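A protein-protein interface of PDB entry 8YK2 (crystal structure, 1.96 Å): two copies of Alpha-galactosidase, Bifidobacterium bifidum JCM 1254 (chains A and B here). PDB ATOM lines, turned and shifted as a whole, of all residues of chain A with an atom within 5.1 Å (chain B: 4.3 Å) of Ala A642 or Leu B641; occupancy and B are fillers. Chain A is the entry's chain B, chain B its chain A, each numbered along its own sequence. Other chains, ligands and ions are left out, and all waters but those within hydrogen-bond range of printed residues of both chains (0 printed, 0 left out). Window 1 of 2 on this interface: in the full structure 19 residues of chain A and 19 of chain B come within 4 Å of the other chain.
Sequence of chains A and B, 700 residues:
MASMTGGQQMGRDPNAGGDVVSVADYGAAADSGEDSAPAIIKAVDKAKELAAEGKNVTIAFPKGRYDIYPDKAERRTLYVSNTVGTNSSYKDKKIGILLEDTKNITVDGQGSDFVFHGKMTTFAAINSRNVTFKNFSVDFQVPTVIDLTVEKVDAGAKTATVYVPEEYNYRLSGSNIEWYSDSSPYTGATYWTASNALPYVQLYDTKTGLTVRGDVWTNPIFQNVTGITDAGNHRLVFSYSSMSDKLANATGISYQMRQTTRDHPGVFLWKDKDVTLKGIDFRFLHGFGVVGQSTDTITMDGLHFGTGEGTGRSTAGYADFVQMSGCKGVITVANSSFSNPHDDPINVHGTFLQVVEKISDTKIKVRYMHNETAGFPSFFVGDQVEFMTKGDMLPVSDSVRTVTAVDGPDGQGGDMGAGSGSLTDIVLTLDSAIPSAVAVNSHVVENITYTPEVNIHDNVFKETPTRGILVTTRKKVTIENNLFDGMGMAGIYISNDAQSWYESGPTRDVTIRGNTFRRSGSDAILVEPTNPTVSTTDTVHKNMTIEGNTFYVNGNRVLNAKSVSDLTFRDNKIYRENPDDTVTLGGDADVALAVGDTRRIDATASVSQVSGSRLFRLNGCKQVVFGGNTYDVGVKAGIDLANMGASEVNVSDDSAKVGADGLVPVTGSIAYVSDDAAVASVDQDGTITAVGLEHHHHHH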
ATOM      1  N   ARG A 617     -12.065 -10.600 -22.627  1.00  0.00           N
ATOM      2  CA  ARG A 617     -10.813 -11.070 -22.045  1.00  0.00           C
ATOM      3  C   ARG A 617      -9.791  -9.953 -22.154  1.00  0.00           C
ATOM      4  O   ARG A 617      -9.673  -9.318 -23.203  1.00  0.00           O
ATOM      5  CB  ARG A 617     -10.280 -12.331 -22.741  1.00  0.00           C
ATOM      6  CG  ARG A 617      -8.945 -12.822 -22.180  1.00  0.00           C
ATOM      7  CD  ARG A 617      -8.524 -14.177 -22.766  1.00  0.00           C
ATOM      8  NE  ARG A 617      -7.195 -14.574 -22.290  1.00  0.00           N
ATOM      9  CZ  ARG A 617      -6.053 -14.220 -22.867  1.00  0.00           C
ATOM     10  NH1 ARG A 617      -6.032 -13.453 -23.950  1.00  0.00           N
ATOM     11  NH2 ARG A 617      -4.901 -14.651 -22.350  1.00  0.00           N
ATOM     12  N   LEU A 618      -9.058  -9.718 -21.072  1.00  0.00           N
ATOM     13  CA  LEU A 618      -8.035  -8.683 -21.038  1.00  0.00           C
ATOM     14  C   LEU A 618      -6.751  -9.329 -20.545  1.00  0.00           C
ATOM     15  O   LEU A 618      -6.776 -10.088 -19.575  1.00  0.00           O
ATOM     16  CB  LEU A 618      -8.448  -7.529 -20.119  1.00  0.00           C
ATOM     17  CG  LEU A 618      -9.813  -6.880 -20.395  1.00  0.00           C
ATOM     18  CD1 LEU A 618     -10.208  -5.927 -19.244  1.00  0.00           C
ATOM     19  CD2 LEU A 618      -9.794  -6.144 -21.738  1.00  0.00           C
ATOM     20  N   ASN A 619      -5.642  -9.030 -21.207  1.00  0.00           N
ATOM     21  CA  ASN A 619      -4.365  -9.679 -20.929  1.00  0.00           C
ATOM     22  C   ASN A 619      -3.312  -8.586 -20.800  1.00  0.00           C
ATOM     23  O   ASN A 619      -2.916  -7.993 -21.806  1.00  0.00           O
ATOM     24  CB  ASN A 619      -3.994 -10.667 -22.040  1.00  0.00           C
ATOM     25  CG  ASN A 619      -2.655 -11.353 -21.779  1.00  0.00           C
ATOM     26  OD1 ASN A 619      -2.085 -11.222 -20.694  1.00  0.00           O
ATOM     27  ND2 ASN A 619      -2.164 -12.101 -22.763  1.00  0.00           N
ATOM     28  N   GLY A 620      -2.870  -8.308 -19.572  1.00  0.00           N
ATOM     29  CA  GLY A 620      -1.835  -7.299 -19.401  1.00  0.00           C
ATOM     30  C   GLY A 620      -2.246  -5.898 -19.810  1.00  0.00           C
ATOM     31  O   GLY A 620      -1.413  -5.137 -20.305  1.00  0.00           O
ATOM     32  N   ASP A 640     -12.623 -12.205 -18.419  1.00  0.00           N
ATOM     33  CA  ASP A 640     -11.469 -13.005 -18.022  1.00  0.00           C
ATOM     34  C   ASP A 640     -10.236 -12.111 -17.958  1.00  0.00           C
ATOM     35  O   ASP A 640     -10.025 -11.269 -18.833  1.00  0.00           O
ATOM     36  CB  ASP A 640     -11.214 -14.144 -19.016  1.00  0.00           C
ATOM     37  CG  ASP A 640     -12.266 -15.246 -18.944  1.00  0.00           C
ATOM     38  OD1 ASP A 640     -12.537 -15.755 -17.832  1.00  0.00           O
ATOM     39  OD2 ASP A 640     -12.814 -15.606 -20.014  1.00  0.00           O
ATOM     40  N   LEU A 641      -9.417 -12.299 -16.928  1.00  0.00           N
ATOM     41  CA  LEU A 641      -8.213 -11.498 -16.740  1.00  0.00           C
ATOM     42  C   LEU A 641      -6.989 -12.396 -16.800  1.00  0.00           C
ATOM     43  O   LEU A 641      -6.952 -13.437 -16.141  1.00  0.00           O
ATOM     44  CB  LEU A 641      -8.221 -10.768 -15.390  1.00  0.00           C
ATOM     45  CG  LEU A 641      -9.355  -9.776 -15.126  1.00  0.00           C
ATOM     46  CD1 LEU A 641      -9.113  -9.107 -13.769  1.00  0.00           C
ATOM     47  CD2 LEU A 641      -9.414  -8.747 -16.242  1.00  0.00           C
ATOM     48  N   ALA A 642      -5.984 -11.971 -17.558  1.00  0.00           N
ATOM     49  CA  ALA A 642      -4.665 -12.587 -17.527  1.00  0.00           C
ATOM     50  C   ALA A 642      -3.637 -11.487 -17.304  1.00  0.00           C
ATOM     51  O   ALA A 642      -3.786 -10.379 -17.832  1.00  0.00           O
ATOM     52  CB  ALA A 642      -4.369 -13.346 -18.840  1.00  0.00           C
ATOM     53  N   ASN A 643      -2.612 -11.776 -16.491  1.00  0.00           N
ATOM     54  CA  ASN A 643      -1.487 -10.851 -16.304  1.00  0.00           C
ATOM     55  C   ASN A 643      -1.936  -9.457 -15.866  1.00  0.00           C
ATOM     56  O   ASN A 643      -1.357  -8.451 -16.283  1.00  0.00           O
ATOM     57  CB  ASN A 643      -0.650 -10.750 -17.584  1.00  0.00           C
ATOM     58  CG  ASN A 643       0.036 -12.051 -17.925  1.00  0.00           C
ATOM     59  OD1 ASN A 643      -0.136 -12.604 -19.022  1.00  0.00           O
ATOM     60  ND2 ASN A 643       0.800 -12.567 -16.978  1.00  0.00           N
ATOM     61  N   MET A 644      -2.968  -9.391 -15.024  1.00  0.00           N
ATOM     62  CA  MET A 644      -3.466  -8.108 -14.538  1.00  0.00           C
ATOM     63  C   MET A 644      -4.502  -8.375 -13.462  1.00  0.00           C
ATOM     64  O   MET A 644      -5.137  -9.434 -13.431  1.00  0.00           O
ATOM     65  CB  MET A 644      -4.090  -7.269 -15.659  1.00  0.00           C
ATOM     66  CG  MET A 644      -5.305  -7.950 -16.273  1.00  0.00           C
ATOM     67  SD  MET A 644      -5.946  -7.022 -17.671  1.00  0.00           S
ATOM     68  CE  MET A 644      -6.592  -5.502 -16.960  1.00  0.00           C
ATOM     69  N   LEU B 618      -0.573 -19.131 -11.442  1.00  0.00           N
ATOM     70  CA  LEU B 618      -1.290 -18.622 -10.281  1.00  0.00           C
ATOM     71  C   LEU B 618      -2.559 -17.945 -10.775  1.00  0.00           C
ATOM     72  O   LEU B 618      -2.528 -17.187 -11.750  1.00  0.00           O
ATOM     73  CB  LEU B 618      -0.431 -17.618  -9.483  1.00  0.00           C
ATOM     74  CG  LEU B 618       1.000 -18.090  -9.167  1.00  0.00           C
ATOM     75  CD1 LEU B 618       1.849 -16.922  -8.660  1.00  0.00           C
ATOM     76  CD2 LEU B 618       0.939 -19.202  -8.121  1.00  0.00           C
ATOM     77  N   ILE B 639       6.024 -17.880 -14.834  1.00  0.00           N
ATOM     78  CA  ILE B 639       4.773 -17.857 -14.080  1.00  0.00           C
ATOM     79  C   ILE B 639       3.679 -17.249 -14.952  1.00  0.00           C
ATOM     80  O   ILE B 639       3.767 -16.077 -15.339  1.00  0.00           O
ATOM     81  CB  ILE B 639       4.909 -17.075 -12.756  1.00  0.00           C
ATOM     82  CG1 ILE B 639       6.106 -17.592 -11.937  1.00  0.00           C
ATOM     83  CG2 ILE B 639       3.619 -17.210 -11.927  1.00  0.00           C
ATOM     84  CD1 ILE B 639       6.491 -16.693 -10.733  1.00  0.00           C
ATOM     85  N   ASP B 640       2.662 -18.053 -15.273  1.00  0.00           N
ATOM     86  CA  ASP B 640       1.435 -17.550 -15.879  1.00  0.00           C
ATOM     87  C   ASP B 640       0.517 -16.982 -14.803  1.00  0.00           C
ATOM     88  O   ASP B 640       0.324 -17.600 -13.754  1.00  0.00           O
ATOM     89  CB  ASP B 640       0.697 -18.675 -16.604  1.00  0.00           C
ATOM     90  CG  ASP B 640       1.382 -19.094 -17.887  1.00  0.00           C
ATOM     91  OD1 ASP B 640       1.657 -18.206 -18.715  1.00  0.00           O
ATOM     92  OD2 ASP B 640       1.634 -20.308 -18.062  1.00  0.00           O
ATOM     93  N   LEU B 641      -0.093 -15.833 -15.082  1.00  0.00           N
ATOM     94  CA  LEU B 641      -0.949 -15.161 -14.113  1.00  0.00           C
ATOM     95  C   LEU B 641      -2.361 -15.058 -14.663  1.00  0.00           C
ATOM     96  O   LEU B 641      -2.558 -14.574 -15.782  1.00  0.00           O
ATOM     97  CB  LEU B 641      -0.434 -13.752 -13.789  1.00  0.00           C
ATOM     98  CG  LEU B 641       0.875 -13.578 -13.005  1.00  0.00           C
ATOM     99  CD1 LEU B 641       1.063 -12.097 -12.690  1.00  0.00           C
ATOM    100  CD2 LEU B 641       0.855 -14.402 -11.728  1.00  0.00           C
ATOM    101  N   ALA B 642      -3.336 -15.497 -13.871  1.00  0.00           N
ATOM    102  CA  ALA B 642      -4.746 -15.298 -14.174  1.00  0.00           C
ATOM    103  C   ALA B 642      -5.404 -14.579 -13.008  1.00  0.00           C
ATOM    104  O   ALA B 642      -5.111 -14.869 -11.847  1.00  0.00           O
ATOM    105  CB  ALA B 642      -5.461 -16.626 -14.428  1.00  0.00           C
ATOM    106  N   MET B 644      -5.043 -11.819 -11.633  1.00  0.00           N
ATOM    107  CA  MET B 644      -4.120 -11.192 -10.698  1.00  0.00           C
ATOM    108  C   MET B 644      -2.957 -10.607 -11.482  1.00  0.00           C
ATOM    109  O   MET B 644      -2.628 -11.084 -12.575  1.00  0.00           O
ATOM    110  CB  MET B 644      -3.599 -12.201  -9.674  1.00  0.00           C
ATOM    111  CG  MET B 644      -2.716 -13.272 -10.314  1.00  0.00           C
ATOM    112  SD  MET B 644      -2.127 -14.469  -9.110  1.00  0.00           S
ATOM    113  CE  MET B 644      -1.182 -13.471  -7.968  1.00  0.00           C
ATOM    114  N   GLY B 645      -2.345  -9.568 -10.907  1.00  0.00           N
ATOM    115  CA  GLY B 645      -1.194  -8.913 -11.482  1.00  0.00           C
ATOM    116  C   GLY B 645       0.088  -9.244 -10.726  1.00  0.00           C
ATOM    117  O   GLY B 645       0.094  -9.913  -9.697  1.00  0.00           O
ATOM    118  N   ALA B 646       1.198  -8.732 -11.264  1.00  0.00           N
ATOM    119  CA  ALA B 646       2.515  -9.121 -10.766  1.00  0.00           C
ATOM    120  C   ALA B 646       2.800  -8.599  -9.364  1.00  0.00           C
ATOM    121  O   ALA B 646       3.705  -9.115  -8.703  1.00  0.00           O
ATOM    122  CB  ALA B 646       3.604  -8.627 -11.719  1.00  0.00           C
ATOM    123  N   VAL B 649       3.112 -11.138  -6.475  1.00  0.00           N
ATOM    124  CA  VAL B 649       4.082 -12.225  -6.604  1.00  0.00           C
ATOM    125  C   VAL B 649       5.481 -11.666  -6.361  1.00  0.00           C
ATOM    126  O   VAL B 649       5.954 -10.808  -7.118  1.00  0.00           O
ATOM    127  CB  VAL B 649       4.008 -12.900  -7.983  1.00  0.00           C
ATOM    128  CG1 VAL B 649       4.849 -14.170  -7.992  1.00  0.00           C
ATOM    129  CG2 VAL B 649       2.552 -13.196  -8.365  1.00  0.00           C
ATOM    130  N   VAL B 658       7.952 -13.645 -13.706  1.00  0.00           N
ATOM    131  CA  VAL B 658       6.517 -13.396 -13.793  1.00  0.00           C
ATOM    132  C   VAL B 658       6.169 -12.928 -15.201  1.00  0.00           C
ATOM    133  O   VAL B 658       6.755 -11.965 -15.714  1.00  0.00           O
ATOM    134  CB  VAL B 658       6.085 -12.358 -12.748  1.00  0.00           C
ATOM    135  CG1 VAL B 658       4.602 -12.019 -12.904  1.00  0.00           C
ATOM    136  CG2 VAL B 658       6.389 -12.862 -11.336  1.00  0.00           C
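The backbone NH (N) of Asn A643 is in hydrogen-bond range of the backbone carbonyl oxygen (O) of Leu B641 (2.9 Å).
The backbone carbonyl oxygen of Met A644 sits at hydrogen-bond distance from the backbone NH of Met B644, 3.0 Å away.
The backbone carbonyl oxygen (O) of Leu A618 is in hydrogen-bond range of the backbone NH (N) of Ala A642.
The side-chain amide oxygen of Asn A619 sits close to the backbone carbonyl oxygen of Ala A642 (3.4 Å).
The side-chain amide oxygen of Asn A619 sits close to the side-chain amide oxygen of Asn A643, 2.9 Å away.
The backbone NH (N) of Gly A620 sits at hydrogen-bond distance from the backbone carbonyl oxygen (O) of Ala A642 (2.9 Å).
O of Leu B618 sits at hydrogen-bond distance from N of Ala B642 (2.8 Å).
Among the printed residues, pairs that only touch across the chains: Leu A641 with Ala B642 (3.5 Å), Ala A642 with Leu B641 (3.4 Å), Asn A643 with Met B644 (3.7 Å) and Met A644 with Gly B645 (3.6 Å).
Of chain B, only Leu B641 (3.4 Å) comes within 4 Å of Ala A642.
Of chain A, only Ala A642 (3.4 Å) and Asn A643 (2.9 Å) come within 4 Å of Leu B641.
Of the printed residues of chain B, Asn A643 touches Leu B641 and Met B644.
Of the printed residues of chain A, Gly B645 touches Met A644 (3.6 Å).
Of the printed residues of chain B, Leu A641 touches Ala B642 (3.5 Å).
Of the printed residues of chain A, Ala B642 touches Leu A641.
Of the printed residues of chain A, Met B644 touches Asn A643 and Met A644.
The nearest printed residue of chain B that does not touch Asn A643 is Gly B645 (4.5 Å).
Hydrophobic or aromatic side chains of chain B that line the printed part of chain A: Leu B641 and Ala B642.
Among the printed residues, no Asp or Glu carboxylate lies within 4 Å of a Lys or Arg side-chain nitrogen of the other chain.
Leu A641 touches Ala B642, and with the chains exchanged Ala A642 touches Leu B641.
Met A644 touches its own counterpart, Met B644.
Positions printed for both chains: 618, 640, 641, 642 and 644.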
